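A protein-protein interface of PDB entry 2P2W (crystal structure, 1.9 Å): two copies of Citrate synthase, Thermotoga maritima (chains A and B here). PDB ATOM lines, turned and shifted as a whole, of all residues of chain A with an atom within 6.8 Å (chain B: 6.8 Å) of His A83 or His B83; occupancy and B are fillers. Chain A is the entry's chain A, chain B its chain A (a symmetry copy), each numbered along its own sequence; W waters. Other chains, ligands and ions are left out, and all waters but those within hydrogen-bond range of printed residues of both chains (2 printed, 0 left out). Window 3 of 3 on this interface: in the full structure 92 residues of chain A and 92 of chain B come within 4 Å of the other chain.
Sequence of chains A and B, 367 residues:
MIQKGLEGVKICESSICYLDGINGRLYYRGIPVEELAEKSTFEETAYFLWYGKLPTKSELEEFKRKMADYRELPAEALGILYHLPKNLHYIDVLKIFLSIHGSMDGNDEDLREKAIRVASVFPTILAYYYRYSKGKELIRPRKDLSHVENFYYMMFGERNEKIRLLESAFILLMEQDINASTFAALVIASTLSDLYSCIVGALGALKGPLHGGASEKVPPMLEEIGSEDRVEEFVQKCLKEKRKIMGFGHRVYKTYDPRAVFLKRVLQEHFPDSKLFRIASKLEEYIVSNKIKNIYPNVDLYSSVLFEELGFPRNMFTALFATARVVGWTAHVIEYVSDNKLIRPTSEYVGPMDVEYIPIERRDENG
A ring nitrogen (NE2) of His B83 lies close to a ring nitrogen (NE2) of His A83, 3.0 Å away.
The backbone carbonyl oxygen (O) of Gly A79 sits at hydrogen-bond distance from a ring nitrogen (ND1) of His A83. The backbone carbonyl oxygen of Leu A84 lies within hydrogen-bond range of the side-chain hydroxyl of Tyr A132, 2.7 Å away. The backbone carbonyl oxygen (O) of Gly B79 sits at hydrogen-bond distance from a ring nitrogen (ND1) of His B83. The backbone carbonyl oxygen (O) of Leu B84 lies within hydrogen-bond range of the side-chain hydroxyl (OH) of Tyr B132.
Glu A76 touches Pro B85 (OE1 to CG, 3.6 Å). Ile A80 touches His B83 (CG1 to O, 3.5 Å). Ile A80 touches Leu B84. Ile B80 touches His A83. Ile B80 touches Leu A84 (CD1 to CD2, 3.8 Å). CG of Pro A85 touches OE1 of Glu B76 (3.6 Å).
Of the printed residues of chain B, Glu A76 touches Pro B85 (3.6 Å). His A83 touches just these residues of chain B: Ile B80 (3.5 Å) and His B83 (3.0 Å). Of the printed residues of chain B, Leu A84 touches Ile B80 (3.8 Å). Of chain A, only Ile A80 (3.5 Å) and His A83 (3.0 Å) come within 4 Å of His B83. Of the printed residues of chain A, Leu B84 touches Ile A80 (3.8 Å). Printed residues of chain A within 4 Å of Pro B85: Glu A76. The nearest residue of chain B that does not touch His A83 is Glu B76 (4.6 Å).
Of the 11 printed residues of chain A, 5 touch a printed residue of chain B. Printed residues of chain A that touch a printed residue of chain B: Glu A76, Ile A80, His A83, Leu A84 and Pro A85. Among the printed residues, 7 pairs touch across the chains. Among the printed residues, no Asp or Glu carboxylate lies within 4 Å of a Lys or Arg side-chain nitrogen of the other chain.
Glu A76 touches Pro B85, and with the chains exchanged Pro A85 touches Glu B76. Ile A80 touches His B83, and with the chains exchanged His A83 touches Ile B80. Ile A80 touches Leu B84, and with the chains exchanged Leu A84 touches Ile B80. His B83 touches its own counterpart, His A83. 11 positions are printed for both chains.
Water W1 lies within hydrogen-bond range of the backbone carbonyl oxygen (O) of His B83 (2.7 Å) and the backbone carbonyl oxygen (O) of Glu A76 (2.9 Å). Water W2 bridges the backbone carbonyl oxygen of His A83 (2.7 Å) and the backbone carbonyl oxygen of Glu B76 (2.9 Å).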
ATOM      1  N   GLU A  76     -14.191   7.478 -12.221  1.00  0.00           N
ATOM      2  CA  GLU A  76     -13.611   7.324 -13.551  1.00  0.00           C
ATOM      3  C   GLU A  76     -13.474   5.854 -13.942  1.00  0.00           C
ATOM      4  O   GLU A  76     -13.638   5.496 -15.109  1.00  0.00           O
ATOM      5  CB  GLU A  76     -12.243   8.004 -13.609  1.00  0.00           C
ATOM      6  CG  GLU A  76     -11.165   7.296 -12.813  1.00  0.00           C
ATOM      7  CD  GLU A  76     -10.044   8.228 -12.405  1.00  0.00           C
ATOM      8  OE1 GLU A  76     -10.036   9.388 -12.873  1.00  0.00           O
ATOM      9  OE2 GLU A  76      -9.175   7.803 -11.612  1.00  0.00           O
ATOM     10  N   ALA A  77     -13.174   5.007 -12.963  1.00  0.00           N
ATOM     11  CA  ALA A  77     -13.028   3.579 -13.218  1.00  0.00           C
ATOM     12  C   ALA A  77     -14.363   3.027 -13.689  1.00  0.00           C
ATOM     13  O   ALA A  77     -14.423   2.190 -14.588  1.00  0.00           O
ATOM     14  CB  ALA A  77     -12.580   2.861 -11.949  1.00  0.00           C
ATOM     15  N   LEU A  78     -15.439   3.509 -13.079  1.00  0.00           N
ATOM     16  CA  LEU A  78     -16.768   3.057 -13.441  1.00  0.00           C
ATOM     17  C   LEU A  78     -17.051   3.422 -14.895  1.00  0.00           C
ATOM     18  O   LEU A  78     -17.689   2.666 -15.624  1.00  0.00           O
ATOM     19  CB  LEU A  78     -17.805   3.691 -12.512  1.00  0.00           C
ATOM     20  CG  LEU A  78     -19.006   2.802 -12.192  1.00  0.00           C
ATOM     21  CD1 LEU A  78     -18.514   1.453 -11.681  1.00  0.00           C
ATOM     22  CD2 LEU A  78     -19.890   3.480 -11.152  1.00  0.00           C
ATOM     23  N   GLY A  79     -16.561   4.583 -15.316  1.00  0.00           N
ATOM     24  CA  GLY A  79     -16.766   5.009 -16.689  1.00  0.00           C
ATOM     25  C   GLY A  79     -16.110   4.048 -17.664  1.00  0.00           C
ATOM     26  O   GLY A  79     -16.681   3.712 -18.703  1.00  0.00           O
ATOM     27  N   ILE A  80     -14.904   3.605 -17.325  1.00  0.00           N
ATOM     28  CA  ILE A  80     -14.155   2.670 -18.157  1.00  0.00           C
ATOM     29  C   ILE A  80     -14.844   1.307 -18.214  1.00  0.00           C
ATOM     30  O   ILE A  80     -14.889   0.673 -19.264  1.00  0.00           O
ATOM     31  CB  ILE A  80     -12.721   2.492 -17.610  1.00  0.00           C
ATOM     32  CG1 ILE A  80     -11.887   3.728 -17.948  1.00  0.00           C
ATOM     33  CG2 ILE A  80     -12.090   1.231 -18.169  1.00  0.00           C
ATOM     34  CD1 ILE A  80     -10.867   4.089 -16.885  1.00  0.00           C
ATOM     35  N   LEU A  81     -15.379   0.865 -17.079  1.00  0.00           N
ATOM     36  CA  LEU A  81     -16.059  -0.428 -16.995  1.00  0.00           C
ATOM     37  C   LEU A  81     -17.109  -0.633 -18.081  1.00  0.00           C
ATOM     38  O   LEU A  81     -17.136  -1.670 -18.749  1.00  0.00           O
ATOM     39  CB  LEU A  81     -16.730  -0.587 -15.628  1.00  0.00           C
ATOM     40  CG  LEU A  81     -17.597  -1.839 -15.452  1.00  0.00           C
ATOM     41  CD1 LEU A  81     -16.718  -3.077 -15.475  1.00  0.00           C
ATOM     42  CD2 LEU A  81     -18.369  -1.761 -14.146  1.00  0.00           C
ATOM     43  N   TYR A  82     -17.967   0.365 -18.258  1.00  0.00           N
ATOM     44  CA  TYR A  82     -19.074   0.257 -19.210  1.00  0.00           C
ATOM     45  C   TYR A  82     -18.640   0.345 -20.691  1.00  0.00           C
ATOM     46  O   TYR A  82     -19.459   0.322 -21.603  1.00  0.00           O
ATOM     47  CB  TYR A  82     -20.123   1.329 -18.877  1.00  0.00           C
ATOM     48  CG  TYR A  82     -20.979   0.856 -17.746  1.00  0.00           C
ATOM     49  CD1 TYR A  82     -21.948  -0.120 -17.963  1.00  0.00           C
ATOM     50  CD2 TYR A  82     -20.790   1.359 -16.456  1.00  0.00           C
ATOM     51  CE1 TYR A  82     -22.707  -0.606 -16.903  1.00  0.00           C
ATOM     52  CE2 TYR A  82     -21.553   0.880 -15.396  1.00  0.00           C
ATOM     53  CZ  TYR A  82     -22.510  -0.098 -15.617  1.00  0.00           C
ATOM     54  OH  TYR A  82     -23.263  -0.593 -14.566  1.00  0.00           O
ATOM     55  N   HIS A  83     -17.310   0.474 -20.924  1.00  0.00           N
ATOM     56  CA  HIS A  83     -16.817   0.500 -22.304  1.00  0.00           C
ATOM     57  C   HIS A  83     -15.898  -0.707 -22.592  1.00  0.00           C
ATOM     58  O   HIS A  83     -15.256  -0.799 -23.629  1.00  0.00           O
ATOM     59  CB  HIS A  83     -16.039   1.807 -22.541  1.00  0.00           C
ATOM     60  CG  HIS A  83     -16.970   3.004 -22.505  1.00  0.00           C
ATOM     61  ND1 HIS A  83     -17.120   3.786 -21.403  1.00  0.00           N
ATOM     62  CD2 HIS A  83     -17.791   3.511 -23.525  1.00  0.00           C
ATOM     63  CE1 HIS A  83     -18.030   4.722 -21.755  1.00  0.00           C
ATOM     64  NE2 HIS A  83     -18.450   4.583 -23.019  1.00  0.00           N
ATOM     65  N   LEU A  84     -15.817  -1.620 -21.592  1.00  0.00           N
ATOM     66  CA  LEU A  84     -14.975  -2.820 -21.750  1.00  0.00           C
ATOM     67  C   LEU A  84     -15.759  -3.965 -22.399  1.00  0.00           C
ATOM     68  O   LEU A  84     -16.979  -4.031 -22.336  1.00  0.00           O
ATOM     69  CB  LEU A  84     -14.562  -3.322 -20.370  1.00  0.00           C
ATOM     70  CG  LEU A  84     -13.552  -2.470 -19.594  1.00  0.00           C
ATOM     71  CD1 LEU A  84     -13.291  -3.089 -18.226  1.00  0.00           C
ATOM     72  CD2 LEU A  84     -12.188  -2.363 -20.287  1.00  0.00           C
ATOM     73  N   PRO A  85     -15.034  -4.891 -23.044  1.00  0.00           N
ATOM     74  CA  PRO A  85     -15.709  -6.032 -23.666  1.00  0.00           C
ATOM     75  C   PRO A  85     -16.307  -6.815 -22.498  1.00  0.00           C
ATOM     76  O   PRO A  85     -15.823  -6.704 -21.372  1.00  0.00           O
ATOM     77  CB  PRO A  85     -14.563  -6.787 -24.335  1.00  0.00           C
ATOM     78  CG  PRO A  85     -13.594  -5.699 -24.673  1.00  0.00           C
ATOM     79  CD  PRO A  85     -13.613  -4.844 -23.429  1.00  0.00           C
ATOM     80  N   TYR A 132     -21.917  -6.371 -14.637  1.00  0.00           N
ATOM     81  CA  TYR A 132     -21.846  -5.665 -15.909  1.00  0.00           C
ATOM     82  C   TYR A 132     -21.863  -6.623 -17.095  1.00  0.00           C
ATOM     83  O   TYR A 132     -22.680  -6.481 -18.005  1.00  0.00           O
ATOM     84  CB  TYR A 132     -20.576  -4.811 -15.961  1.00  0.00           C
ATOM     85  CG  TYR A 132     -20.204  -4.342 -17.349  1.00  0.00           C
ATOM     86  CD1 TYR A 132     -21.018  -3.449 -18.049  1.00  0.00           C
ATOM     87  CD2 TYR A 132     -19.039  -4.795 -17.967  1.00  0.00           C
ATOM     88  CE1 TYR A 132     -20.678  -3.017 -19.331  1.00  0.00           C
ATOM     89  CE2 TYR A 132     -18.690  -4.375 -19.248  1.00  0.00           C
ATOM     90  CZ  TYR A 132     -19.515  -3.484 -19.924  1.00  0.00           C
ATOM     91  OH  TYR A 132     -19.170  -3.065 -21.188  1.00  0.00           O
ATOM     92  N   GLU B  76     -12.615  -1.425 -30.276  1.00  0.00           N
ATOM     93  CA  GLU B  76     -13.039  -1.376 -28.880  1.00  0.00           C
ATOM     94  C   GLU B  76     -11.995  -0.700 -27.995  1.00  0.00           C
ATOM     95  O   GLU B  76     -12.338  -0.002 -27.040  1.00  0.00           O
ATOM     96  CB  GLU B  76     -13.318  -2.789 -28.365  1.00  0.00           C
ATOM     97  CG  GLU B  76     -12.076  -3.640 -28.191  1.00  0.00           C
ATOM     98  CD  GLU B  76     -12.379  -5.122 -28.257  1.00  0.00           C
ATOM     99  OE1 GLU B  76     -13.577  -5.482 -28.287  1.00  0.00           O
ATOM    100  OE2 GLU B  76     -11.421  -5.925 -28.285  1.00  0.00           O
ATOM    101  N   ALA B  77     -10.723  -0.911 -28.315  1.00  0.00           N
ATOM    102  CA  ALA B  77      -9.641  -0.308 -27.547  1.00  0.00           C
ATOM    103  C   ALA B  77      -9.733   1.203 -27.673  1.00  0.00           C
ATOM    104  O   ALA B  77      -9.518   1.936 -26.708  1.00  0.00           O
ATOM    105  CB  ALA B  77      -8.291  -0.798 -28.062  1.00  0.00           C
ATOM    106  N   LEU B  78     -10.064   1.666 -28.872  1.00  0.00           N
ATOM    107  CA  LEU B  78     -10.181   3.092 -29.115  1.00  0.00           C
ATOM    108  C   LEU B  78     -11.296   3.666 -28.247  1.00  0.00           C
ATOM    109  O   LEU B  78     -11.192   4.781 -27.742  1.00  0.00           O
ATOM    110  CB  LEU B  78     -10.465   3.345 -30.597  1.00  0.00           C
ATOM    111  CG  LEU B  78      -9.840   4.622 -31.159  1.00  0.00           C
ATOM    112  CD1 LEU B  78      -8.350   4.638 -30.840  1.00  0.00           C
ATOM    113  CD2 LEU B  78     -10.068   4.691 -32.664  1.00  0.00           C
ATOM    114  N   GLY B  79     -12.360   2.890 -28.066  1.00  0.00           N
ATOM    115  CA  GLY B  79     -13.465   3.345 -27.242  1.00  0.00           C
ATOM    116  C   GLY B  79     -13.023   3.568 -25.807  1.00  0.00           C
ATOM    117  O   GLY B  79     -13.410   4.549 -25.170  1.00  0.00           O
ATOM    118  N   ILE B  80     -12.205   2.651 -25.299  1.00  0.00           N
ATOM    119  CA  ILE B  80     -11.690   2.736 -23.937  1.00  0.00           C
ATOM    120  C   ILE B  80     -10.751   3.931 -23.776  1.00  0.00           C
ATOM    121  O   ILE B  80     -10.778   4.613 -22.755  1.00  0.00           O
ATOM    122  CB  ILE B  80     -10.933   1.441 -23.567  1.00  0.00           C
ATOM    123  CG1 ILE B  80     -11.937   0.320 -23.300  1.00  0.00           C
ATOM    124  CG2 ILE B  80     -10.034   1.674 -22.367  1.00  0.00           C
ATOM    125  CD1 ILE B  80     -11.454  -1.052 -23.733  1.00  0.00           C
ATOM    126  N   LEU B  81      -9.924   4.177 -24.788  1.00  0.00           N
ATOM    127  CA  LEU B  81      -8.968   5.285 -24.757  1.00  0.00           C
ATOM    128  C   LEU B  81      -9.599   6.619 -24.374  1.00  0.00           C
ATOM    129  O   LEU B  81      -9.092   7.334 -23.506  1.00  0.00           O
ATOM    130  CB  LEU B  81      -8.288   5.437 -26.119  1.00  0.00           C
ATOM    131  CG  LEU B  81      -7.361   6.649 -26.271  1.00  0.00           C
ATOM    132  CD1 LEU B  81      -6.148   6.481 -25.372  1.00  0.00           C
ATOM    133  CD2 LEU B  81      -6.930   6.800 -27.719  1.00  0.00           C
ATOM    134  N   TYR B  82     -10.710   6.946 -25.022  1.00  0.00           N
ATOM    135  CA  TYR B  82     -11.365   8.238 -24.808  1.00  0.00           C
ATOM    136  C   TYR B  82     -12.101   8.352 -23.454  1.00  0.00           C
ATOM    137  O   TYR B  82     -12.739   9.356 -23.151  1.00  0.00           O
ATOM    138  CB  TYR B  82     -12.320   8.512 -25.980  1.00  0.00           C
ATOM    139  CG  TYR B  82     -11.543   9.038 -27.144  1.00  0.00           C
ATOM    140  CD1 TYR B  82     -11.071  10.348 -27.135  1.00  0.00           C
ATOM    141  CD2 TYR B  82     -11.252   8.212 -28.233  1.00  0.00           C
ATOM    142  CE1 TYR B  82     -10.297  10.825 -28.190  1.00  0.00           C
ATOM    143  CE2 TYR B  82     -10.484   8.689 -29.292  1.00  0.00           C
ATOM    144  CZ  TYR B  82     -10.010   9.991 -29.273  1.00  0.00           C
ATOM    145  OH  TYR B  82      -9.232  10.469 -30.313  1.00  0.00           O
ATOM    146  N   HIS B  83     -12.023   7.277 -22.630  1.00  0.00           N
ATOM    147  CA  HIS B  83     -12.641   7.335 -21.304  1.00  0.00           C
ATOM    148  C   HIS B  83     -11.583   7.212 -20.187  1.00  0.00           C
ATOM    149  O   HIS B  83     -11.892   7.082 -19.011  1.00  0.00           O
ATOM    150  CB  HIS B  83     -13.665   6.193 -21.169  1.00  0.00           C
ATOM    151  CG  HIS B  83     -14.849   6.418 -22.091  1.00  0.00           C
ATOM    152  ND1 HIS B  83     -14.963   5.813 -23.303  1.00  0.00           N
ATOM    153  CD2 HIS B  83     -15.981   7.223 -21.888  1.00  0.00           C
ATOM    154  CE1 HIS B  83     -16.125   6.270 -23.819  1.00  0.00           C
ATOM    155  NE2 HIS B  83     -16.757   7.117 -22.996  1.00  0.00           N
ATOM    156  N   LEU B  84     -10.294   7.206 -20.613  1.00  0.00           N
ATOM    157  CA  LEU B  84      -9.191   7.098 -19.641  1.00  0.00           C
ATOM    158  C   LEU B  84      -8.759   8.479 -19.139  1.00  0.00           C
ATOM    159  O   LEU B  84      -8.951   9.495 -19.794  1.00  0.00           O
ATOM    160  CB  LEU B  84      -7.972   6.502 -20.338  1.00  0.00           C
ATOM    161  CG  LEU B  84      -8.045   5.021 -20.721  1.00  0.00           C
ATOM    162  CD1 LEU B  84      -6.769   4.607 -21.446  1.00  0.00           C
ATOM    163  CD2 LEU B  84      -8.178   4.086 -19.513  1.00  0.00           C
ATOM    164  N   PRO B  85      -8.160   8.516 -17.940  1.00  0.00           N
ATOM    165  CA  PRO B  85      -7.692   9.795 -17.405  1.00  0.00           C
ATOM    166  C   PRO B  85      -6.581  10.235 -18.357  1.00  0.00           C
ATOM    167  O   PRO B  85      -5.982   9.395 -19.030  1.00  0.00           O
ATOM    168  CB  PRO B  85      -7.149   9.417 -16.028  1.00  0.00           C
ATOM    169  CG  PRO B  85      -8.001   8.249 -15.642  1.00  0.00           C
ATOM    170  CD  PRO B  85      -8.071   7.454 -16.923  1.00  0.00           C
ATOM    171  N   TYR B 132      -4.187  11.952 -27.566  1.00  0.00           N
ATOM    172  CA  TYR B 132      -5.409  12.019 -26.776  1.00  0.00           C
ATOM    173  C   TYR B 132      -5.232  12.869 -25.523  1.00  0.00           C
ATOM    174  O   TYR B 132      -6.005  13.796 -25.278  1.00  0.00           O
ATOM    175  CB  TYR B 132      -5.850  10.608 -26.376  1.00  0.00           C
ATOM    176  CG  TYR B 132      -6.867  10.573 -25.258  1.00  0.00           C
ATOM    177  CD1 TYR B 132      -8.151  11.090 -25.438  1.00  0.00           C
ATOM    178  CD2 TYR B 132      -6.543  10.026 -24.016  1.00  0.00           C
ATOM    179  CE1 TYR B 132      -9.090  11.061 -24.406  1.00  0.00           C
ATOM    180  CE2 TYR B 132      -7.471   9.993 -22.978  1.00  0.00           C
ATOM    181  CZ  TYR B 132      -8.743  10.512 -23.181  1.00  0.00           C
ATOM    182  OH  TYR B 132      -9.661  10.479 -22.157  1.00  0.00           O
HETATM  183  O   HOH W   1     -14.046   7.263 -17.341  1.00  0.00           O
HETATM  184  O   HOH W   2     -15.039   0.321 -26.110  1.00  0.00           O
